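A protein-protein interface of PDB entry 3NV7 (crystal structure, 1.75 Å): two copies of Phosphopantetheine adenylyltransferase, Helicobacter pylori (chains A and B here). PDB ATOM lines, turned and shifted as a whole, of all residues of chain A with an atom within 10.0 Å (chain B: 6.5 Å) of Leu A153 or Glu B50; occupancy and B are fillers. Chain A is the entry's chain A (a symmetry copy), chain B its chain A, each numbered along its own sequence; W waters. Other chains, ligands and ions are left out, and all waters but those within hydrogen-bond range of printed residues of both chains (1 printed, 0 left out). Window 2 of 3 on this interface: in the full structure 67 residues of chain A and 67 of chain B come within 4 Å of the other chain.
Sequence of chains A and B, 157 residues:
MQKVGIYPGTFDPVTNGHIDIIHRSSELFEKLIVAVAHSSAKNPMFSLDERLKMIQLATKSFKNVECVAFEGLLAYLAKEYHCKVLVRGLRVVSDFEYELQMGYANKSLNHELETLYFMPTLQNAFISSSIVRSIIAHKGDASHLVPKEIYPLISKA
Water W1 lies within hydrogen-bond range of the side-chain carboxylate of Glu B50 (2.5 Å) and the backbone carbonyl oxygen of Leu A153 (2.7 Å).
Along chain B the printed residues that touch a printed residue of chain A span positions 46 to 57.
Hydrophobic or aromatic side chains of chain A that line the printed part of chain B: Ile A150 and Ile A154.
Among the printed residues, no Asp or Glu carboxylate lies within 4 Å of a Lys or Arg side-chain nitrogen of the other chain.
No position is printed for both chains.
Among the printed residues, merely in contact across the chains: Glu A149 with Leu B57, Ile A154 with Phe B46, Ile A150 with Met B54, Ile A154 with Met B54 and Leu A153 with Glu B50.
The backbone carbonyl oxygen of Phe B46 sits at hydrogen-bond distance from the guanidinium group of Arg B51 (2.8 Å).
The side-chain hydroxyl (OG) of Ser B47 sits at hydrogen-bond distance from the backbone NH (N) of Glu B50 (3.0 Å).
NZ of Lys A148 lies within salt-bridge range of OE2 of Glu A149.
Of the printed residues of chain B, Leu A153 touches Glu B50 (3.996 Å).
Printed residues of chain A within 4 Å of Glu B50: Leu A153 (3.996 Å).
No residue of chain A comes within 4 Å of Ser B47.
Printed residues of chain B within 4 Å of Glu A149: Leu B57.
Of the printed residues of chain B, Ile A150 touches Met B54.
Printed residues of chain A within 4 Å of Phe B46: Ile A154 (3.5 Å).
Printed residues of chain A within 4 Å of Leu B57: Glu A149.
The nearest printed residue of chain A that does not touch Glu B50 is Ile A154 (5.3 Å).
The nearest printed residue of chain A that does not touch Phe B46 is Leu A153 (4.7 Å).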
ATOM      1  N   VAL A 132      -7.228  -6.108 -12.518  1.00  0.00           N
ATOM      2  CA  VAL A 132      -8.151  -6.839 -13.397  1.00  0.00           C
ATOM      3  C   VAL A 132      -8.317  -8.297 -12.971  1.00  0.00           C
ATOM      4  O   VAL A 132      -9.443  -8.786 -12.921  1.00  0.00           O
ATOM      5  CB  VAL A 132      -7.757  -6.762 -14.906  1.00  0.00           C
ATOM      6  CG1 VAL A 132      -8.588  -7.759 -15.732  1.00  0.00           C
ATOM      7  CG2 VAL A 132      -7.956  -5.342 -15.437  1.00  0.00           C
ATOM      8  N   ILE A 136     -11.698 -10.258 -11.851  1.00  0.00           N
ATOM      9  CA  ILE A 136     -12.052 -11.540 -12.474  1.00  0.00           C
ATOM     10  C   ILE A 136     -12.350 -12.599 -11.407  1.00  0.00           C
ATOM     11  O   ILE A 136     -13.377 -13.282 -11.475  1.00  0.00           O
ATOM     12  CB  ILE A 136     -10.950 -12.033 -13.474  1.00  0.00           C
ATOM     13  CG1 ILE A 136     -10.861 -11.137 -14.724  1.00  0.00           C
ATOM     14  CG2 ILE A 136     -11.154 -13.500 -13.869  1.00  0.00           C
ATOM     15  CD1 ILE A 136     -12.185 -10.450 -15.163  1.00  0.00           C
ATOM     16  N   VAL A 146     -10.468  -3.337 -19.984  1.00  0.00           N
ATOM     17  CA  VAL A 146      -9.710  -4.140 -20.950  1.00  0.00           C
ATOM     18  C   VAL A 146     -10.267  -3.938 -22.357  1.00  0.00           C
ATOM     19  O   VAL A 146     -11.466  -3.593 -22.503  1.00  0.00           O
ATOM     20  CB  VAL A 146      -9.722  -5.660 -20.584  1.00  0.00           C
ATOM     21  CG1 VAL A 146      -8.978  -5.916 -19.288  1.00  0.00           C
ATOM     22  CG2 VAL A 146     -11.184  -6.203 -20.463  1.00  0.00           C
ATOM     23  N   PRO A 147      -9.410  -4.122 -23.396  1.00  0.00           N
ATOM     24  CA  PRO A 147      -9.836  -3.990 -24.792  1.00  0.00           C
ATOM     25  C   PRO A 147     -11.022  -4.913 -25.100  1.00  0.00           C
ATOM     26  O   PRO A 147     -11.079  -6.055 -24.598  1.00  0.00           O
ATOM     27  CB  PRO A 147      -8.592  -4.389 -25.616  1.00  0.00           C
ATOM     28  CG  PRO A 147      -7.488  -4.595 -24.680  1.00  0.00           C
ATOM     29  CD  PRO A 147      -7.967  -4.451 -23.267  1.00  0.00           C
ATOM     30  N   LYS A 148     -11.969  -4.414 -25.900  1.00  0.00           N
ATOM     31  CA  LYS A 148     -13.181  -5.178 -26.166  1.00  0.00           C
ATOM     32  C   LYS A 148     -12.895  -6.478 -26.895  1.00  0.00           C
ATOM     33  O   LYS A 148     -13.663  -7.432 -26.801  1.00  0.00           O
ATOM     34  CB  LYS A 148     -14.206  -4.338 -26.921  1.00  0.00           C
ATOM     35  CG  LYS A 148     -13.776  -3.850 -28.273  1.00  0.00           C
ATOM     36  CD  LYS A 148     -14.979  -3.150 -28.950  1.00  0.00           C
ATOM     37  CE  LYS A 148     -14.570  -2.394 -30.213  1.00  0.00           C
ATOM     38  NZ  LYS A 148     -13.983  -3.298 -31.248  1.00  0.00           N
ATOM     39  N   GLU A 149     -11.764  -6.524 -27.586  1.00  0.00           N
ATOM     40  CA  GLU A 149     -11.363  -7.688 -28.368  1.00  0.00           C
ATOM     41  C   GLU A 149     -11.104  -8.900 -27.483  1.00  0.00           C
ATOM     42  O   GLU A 149     -11.293 -10.033 -27.921  1.00  0.00           O
ATOM     43  CB  GLU A 149     -10.104  -7.394 -29.202  1.00  0.00           C
ATOM     44  CG  GLU A 149     -10.287  -6.425 -30.355  1.00  0.00           C
ATOM     45  CD  GLU A 149     -10.195  -4.967 -29.942  1.00  0.00           C
ATOM     46  OE1 GLU A 149      -9.811  -4.683 -28.799  1.00  0.00           O
ATOM     47  OE2 GLU A 149     -10.527  -4.096 -30.772  1.00  0.00           O
ATOM     48  N   ILE A 150     -10.689  -8.658 -26.239  1.00  0.00           N
ATOM     49  CA  ILE A 150     -10.339  -9.743 -25.322  1.00  0.00           C
ATOM     50  C   ILE A 150     -11.359 -10.006 -24.212  1.00  0.00           C
ATOM     51  O   ILE A 150     -11.262 -11.031 -23.537  1.00  0.00           O
ATOM     52  CB  ILE A 150      -8.916  -9.561 -24.657  1.00  0.00           C
ATOM     53  CG1 ILE A 150      -8.981  -8.609 -23.449  1.00  0.00           C
ATOM     54  CG2 ILE A 150      -7.858  -9.155 -25.687  1.00  0.00           C
ATOM     55  CD1 ILE A 150      -7.968  -8.900 -22.366  1.00  0.00           C
ATOM     56  N   TYR A 151     -12.310  -9.095 -23.990  1.00  0.00           N
ATOM     57  CA  TYR A 151     -13.200  -9.260 -22.835  1.00  0.00           C
ATOM     58  C   TYR A 151     -13.939 -10.604 -22.811  1.00  0.00           C
ATOM     59  O   TYR A 151     -13.976 -11.251 -21.756  1.00  0.00           O
ATOM     60  CB  TYR A 151     -14.190  -8.092 -22.647  1.00  0.00           C
ATOM     61  CG  TYR A 151     -14.827  -8.132 -21.260  1.00  0.00           C
ATOM     62  CD1 TYR A 151     -14.022  -8.035 -20.129  1.00  0.00           C
ATOM     63  CD2 TYR A 151     -16.212  -8.324 -21.070  1.00  0.00           C
ATOM     64  CE1 TYR A 151     -14.545  -8.082 -18.837  1.00  0.00           C
ATOM     65  CE2 TYR A 151     -16.770  -8.367 -19.751  1.00  0.00           C
ATOM     66  CZ  TYR A 151     -15.909  -8.239 -18.639  1.00  0.00           C
ATOM     67  OH  TYR A 151     -16.352  -8.275 -17.305  1.00  0.00           O
ATOM     68  N   PRO A 152     -14.521 -11.038 -23.962  1.00  0.00           N
ATOM     69  CA  PRO A 152     -15.209 -12.331 -24.038  1.00  0.00           C
ATOM     70  C   PRO A 152     -14.322 -13.533 -23.705  1.00  0.00           C
ATOM     71  O   PRO A 152     -14.837 -14.634 -23.425  1.00  0.00           O
ATOM     72  CB  PRO A 152     -15.622 -12.435 -25.515  1.00  0.00           C
ATOM     73  CG  PRO A 152     -15.633 -11.063 -26.011  1.00  0.00           C
ATOM     74  CD  PRO A 152     -14.585 -10.315 -25.247  1.00  0.00           C
ATOM     75  N   LEU A 153     -13.005 -13.349 -23.783  1.00  0.00           N
ATOM     76  CA  LEU A 153     -12.075 -14.434 -23.517  1.00  0.00           C
ATOM     77  C   LEU A 153     -11.706 -14.555 -22.042  1.00  0.00           C
ATOM     78  O   LEU A 153     -11.081 -15.540 -21.632  1.00  0.00           O
ATOM     79  CB  LEU A 153     -10.810 -14.253 -24.364  1.00  0.00           C
ATOM     80  CG  LEU A 153     -11.016 -13.977 -25.857  1.00  0.00           C
ATOM     81  CD1 LEU A 153      -9.672 -13.719 -26.530  1.00  0.00           C
ATOM     82  CD2 LEU A 153     -11.758 -15.133 -26.527  1.00  0.00           C
ATOM     83  N   ILE A 154     -12.069 -13.552 -21.249  1.00  0.00           N
ATOM     84  CA  ILE A 154     -11.641 -13.505 -19.844  1.00  0.00           C
ATOM     85  C   ILE A 154     -12.816 -13.368 -18.861  1.00  0.00           C
ATOM     86  O   ILE A 154     -12.630 -13.422 -17.631  1.00  0.00           O
ATOM     87  CB  ILE A 154     -10.547 -12.403 -19.597  1.00  0.00           C
ATOM     88  CG1 ILE A 154     -11.104 -10.991 -19.819  1.00  0.00           C
ATOM     89  CG2 ILE A 154      -9.311 -12.631 -20.463  1.00  0.00           C
ATOM     90  CD1 ILE A 154     -10.192  -9.876 -19.245  1.00  0.00           C
ATOM     91  N   SER A 155     -14.024 -13.237 -19.404  1.00  0.00           N
ATOM     92  CA  SER A 155     -15.229 -13.033 -18.601  1.00  0.00           C
ATOM     93  C   SER A 155     -16.501 -13.448 -19.346  1.00  0.00           C
ATOM     94  O   SER A 155     -16.546 -13.462 -20.580  1.00  0.00           O
ATOM     95  CB  SER A 155     -15.331 -11.572 -18.170  1.00  0.00           C
ATOM     96  OG  SER A 155     -16.612 -11.313 -17.634  1.00  0.00           O
ATOM     97  N   LYS A 156     -17.539 -13.782 -18.587  1.00  0.00           N
ATOM     98  CA  LYS A 156     -18.805 -14.256 -19.158  1.00  0.00           C
ATOM     99  C   LYS A 156     -19.968 -14.064 -18.195  1.00  0.00           C
ATOM    100  O   LYS A 156     -19.750 -13.845 -16.992  1.00  0.00           O
ATOM    101  CB  LYS A 156     -18.702 -15.737 -19.533  1.00  0.00           C
ATOM    102  CG  LYS A 156     -18.504 -16.680 -18.349  1.00  0.00           C
ATOM    103  CD  LYS A 156     -18.306 -18.114 -18.830  1.00  0.00           C
ATOM    104  CE  LYS A 156     -17.763 -18.999 -17.746  1.00  0.00           C
ATOM    105  NZ  LYS A 156     -18.816 -19.319 -16.761  1.00  0.00           N
ATOM    106  N   ALA A 157     -21.188 -14.174 -18.737  1.00  0.00           N
ATOM    107  CA  ALA A 157     -22.454 -14.104 -17.980  1.00  0.00           C
ATOM    108  C   ALA A 157     -22.581 -12.882 -17.058  1.00  0.00           C
ATOM    109  O   ALA A 157     -22.023 -11.807 -17.331  1.00  0.00           O
ATOM    110  CB  ALA A 157     -22.691 -15.408 -17.194  1.00  0.00           C
ATOM    111  N   MET B  45      -1.928 -15.848 -14.637  1.00  0.00           N
ATOM    112  CA  MET B  45      -3.251 -16.443 -14.792  1.00  0.00           C
ATOM    113  C   MET B  45      -3.472 -17.059 -16.171  1.00  0.00           C
ATOM    114  O   MET B  45      -4.035 -18.145 -16.282  1.00  0.00           O
ATOM    115  CB  MET B  45      -4.307 -15.392 -14.526  1.00  0.00           C
ATOM    116  CG  MET B  45      -5.736 -15.863 -14.773  1.00  0.00           C
ATOM    117  SD  MET B  45      -6.892 -14.557 -14.342  1.00  0.00           S
ATOM    118  CE  MET B  45      -6.826 -14.556 -12.562  1.00  0.00           C
ATOM    119  N   PHE B  46      -3.012 -16.375 -17.217  1.00  0.00           N
ATOM    120  CA  PHE B  46      -3.174 -16.836 -18.591  1.00  0.00           C
ATOM    121  C   PHE B  46      -1.836 -17.326 -19.110  1.00  0.00           C
ATOM    122  O   PHE B  46      -0.794 -16.802 -18.707  1.00  0.00           O
ATOM    123  CB  PHE B  46      -3.749 -15.699 -19.470  1.00  0.00           C
ATOM    124  CG  PHE B  46      -5.064 -15.181 -18.965  1.00  0.00           C
ATOM    125  CD1 PHE B  46      -5.126 -13.981 -18.266  1.00  0.00           C
ATOM    126  CD2 PHE B  46      -6.243 -15.952 -19.109  1.00  0.00           C
ATOM    127  CE1 PHE B  46      -6.350 -13.528 -17.723  1.00  0.00           C
ATOM    128  CE2 PHE B  46      -7.485 -15.496 -18.603  1.00  0.00           C
ATOM    129  CZ  PHE B  46      -7.537 -14.292 -17.914  1.00  0.00           C
ATOM    130  N   SER B  47      -1.875 -18.345 -19.975  1.00  0.00           N
ATOM    131  CA  SER B  47      -0.673 -18.935 -20.535  1.00  0.00           C
ATOM    132  C   SER B  47       0.053 -17.909 -21.381  1.00  0.00           C
ATOM    133  O   SER B  47      -0.550 -16.913 -21.828  1.00  0.00           O
ATOM    134  CB  SER B  47      -1.006 -20.147 -21.392  1.00  0.00           C
ATOM    135  OG  SER B  47      -1.706 -19.776 -22.567  1.00  0.00           O
ATOM    136  N   LEU B  48       1.335 -18.151 -21.620  1.00  0.00           N
ATOM    137  CA  LEU B  48       2.086 -17.281 -22.526  1.00  0.00           C
ATOM    138  C   LEU B  48       1.426 -17.200 -23.903  1.00  0.00           C
ATOM    139  O   LEU B  48       1.294 -16.088 -24.457  1.00  0.00           O
ATOM    140  CB  LEU B  48       3.548 -17.740 -22.646  1.00  0.00           C
ATOM    141  CG  LEU B  48       4.427 -16.838 -23.525  1.00  0.00           C
ATOM    142  CD1 LEU B  48       4.316 -15.354 -23.118  1.00  0.00           C
ATOM    143  CD2 LEU B  48       5.878 -17.343 -23.532  1.00  0.00           C
ATOM    144  N   ASP B  49       1.001 -18.348 -24.447  1.00  0.00           N
ATOM    145  CA  ASP B  49       0.344 -18.353 -25.759  1.00  0.00           C
ATOM    146  C   ASP B  49      -0.918 -17.518 -25.756  1.00  0.00           C
ATOM    147  O   ASP B  49      -1.135 -16.721 -26.682  1.00  0.00           O
ATOM    148  CB  ASP B  49      -0.026 -19.769 -26.223  1.00  0.00           C
ATOM    149  CG  ASP B  49      -0.698 -19.772 -27.602  1.00  0.00           C
ATOM    150  OD1 ASP B  49       0.005 -19.469 -28.596  1.00  0.00           O
ATOM    151  OD2 ASP B  49      -1.920 -20.081 -27.698  1.00  0.00           O
ATOM    152  N   GLU B  50      -1.757 -17.691 -24.729  1.00  0.00           N
ATOM    153  CA  GLU B  50      -2.983 -16.888 -24.637  1.00  0.00           C
ATOM    154  C   GLU B  50      -2.670 -15.393 -24.533  1.00  0.00           C
ATOM    155  O   GLU B  50      -3.329 -14.572 -25.163  1.00  0.00           O
ATOM    156  CB  GLU B  50      -3.920 -17.327 -23.476  1.00  0.00           C
ATOM    157  CG  GLU B  50      -5.311 -16.576 -23.589  1.00  0.00           C
ATOM    158  CD  GLU B  50      -6.457 -17.211 -22.833  1.00  0.00           C
ATOM    159  OE1 GLU B  50      -6.233 -18.075 -21.956  1.00  0.00           O
ATOM    160  OE2 GLU B  50      -7.621 -16.849 -23.144  1.00  0.00           O
ATOM    161  N   ARG B  51      -1.669 -15.042 -23.737  1.00  0.00           N
ATOM    162  CA  ARG B  51      -1.361 -13.608 -23.509  1.00  0.00           C
ATOM    163  C   ARG B  51      -0.869 -12.990 -24.806  1.00  0.00           C
ATOM    164  O   ARG B  51      -1.297 -11.893 -25.184  1.00  0.00           O
ATOM    165  CB  ARG B  51      -0.345 -13.442 -22.359  1.00  0.00           C
ATOM    166  CG  ARG B  51      -0.998 -13.689 -21.013  1.00  0.00           C
ATOM    167  CD  ARG B  51      -0.038 -13.561 -19.855  1.00  0.00           C
ATOM    168  NE  ARG B  51       0.860 -14.718 -19.701  1.00  0.00           N
ATOM    169  CZ  ARG B  51       2.197 -14.678 -19.691  1.00  0.00           C
ATOM    170  NH1 ARG B  51       2.856 -13.542 -19.903  1.00  0.00           N
ATOM    171  NH2 ARG B  51       2.888 -15.801 -19.483  1.00  0.00           N
ATOM    172  N   LEU B  52       0.021 -13.697 -25.491  1.00  0.00           N
ATOM    173  CA  LEU B  52       0.515 -13.228 -26.835  1.00  0.00           C
ATOM    174  C   LEU B  52      -0.635 -13.062 -27.830  1.00  0.00           C
ATOM    175  O   LEU B  52      -0.769 -12.035 -28.431  1.00  0.00           O
ATOM    176  CB  LEU B  52       1.493 -14.273 -27.430  1.00  0.00           C
ATOM    177  CG  LEU B  52       2.092 -13.922 -28.798  1.00  0.00           C
ATOM    178  CD1 LEU B  52       2.887 -12.595 -28.759  1.00  0.00           C
ATOM    179  CD2 LEU B  52       2.999 -15.067 -29.324  1.00  0.00           C
ATOM    180  N   LYS B  53      -1.455 -14.110 -27.993  1.00  0.00           N
ATOM    181  CA  LYS B  53      -2.570 -14.031 -28.915  1.00  0.00           C
ATOM    182  C   LYS B  53      -3.557 -12.900 -28.560  1.00  0.00           C
ATOM    183  O   LYS B  53      -4.083 -12.244 -29.445  1.00  0.00           O
ATOM    184  CB  LYS B  53      -3.266 -15.408 -29.025  1.00  0.00           C
ATOM    185  CG  LYS B  53      -2.406 -16.473 -29.684  1.00  0.00           C
ATOM    186  CD  LYS B  53      -2.890 -16.809 -31.056  1.00  0.00           C
ATOM    187  CE  LYS B  53      -2.380 -18.181 -31.502  1.00  0.00           C
ATOM    188  NZ  LYS B  53      -0.915 -18.352 -31.266  1.00  0.00           N
ATOM    189  N   MET B  54      -3.788 -12.652 -27.255  1.00  0.00           N
ATOM    190  CA  MET B  54      -4.742 -11.644 -26.846  1.00  0.00           C
ATOM    191  C   MET B  54      -4.195 -10.267 -27.184  1.00  0.00           C
ATOM    192  O   MET B  54      -4.911  -9.436 -27.717  1.00  0.00           O
ATOM    193  CB  MET B  54      -4.996 -11.734 -25.348  1.00  0.00           C
ATOM    194  CG  MET B  54      -5.861 -12.929 -25.012  1.00  0.00           C
ATOM    195  SD  MET B  54      -6.604 -12.810 -23.381  1.00  0.00           S
ATOM    196  CE  MET B  54      -5.175 -12.823 -22.372  1.00  0.00           C
ATOM    197  N   ILE B  55      -2.920 -10.026 -26.855  1.00  0.00           N
ATOM    198  CA  ILE B  55      -2.362  -8.701 -27.143  1.00  0.00           C
ATOM    199  C   ILE B  55      -2.208  -8.477 -28.666  1.00  0.00           C
ATOM    200  O   ILE B  55      -2.395  -7.351 -29.161  1.00  0.00           O
ATOM    201  CB  ILE B  55      -1.096  -8.395 -26.303  1.00  0.00           C
ATOM    202  CG1 ILE B  55      -0.797  -6.892 -26.360  1.00  0.00           C
ATOM    203  CG2 ILE B  55       0.113  -9.181 -26.798  1.00  0.00           C
ATOM    204  CD1 ILE B  55       0.004  -6.388 -25.165  1.00  0.00           C
ATOM    205  N   LEU B  57      -4.361  -9.709 -30.834  1.00  0.00           N
ATOM    206  CA  LEU B  57      -5.717  -9.421 -31.279  1.00  0.00           C
ATOM    207  C   LEU B  57      -6.074  -7.964 -30.989  1.00  0.00           C
ATOM    208  O   LEU B  57      -6.729  -7.311 -31.791  1.00  0.00           O
ATOM    209  CB  LEU B  57      -6.696 -10.361 -30.580  1.00  0.00           C
ATOM    210  CG  LEU B  57      -8.094 -10.530 -31.171  1.00  0.00           C
ATOM    211  CD1 LEU B  57      -8.024 -11.215 -32.543  1.00  0.00           C
ATOM    212  CD2 LEU B  57      -8.950 -11.317 -30.178  1.00  0.00           C
HETATM  213  O   HOH W   1      -9.799 -17.797 -22.328  1.00  0.00           O
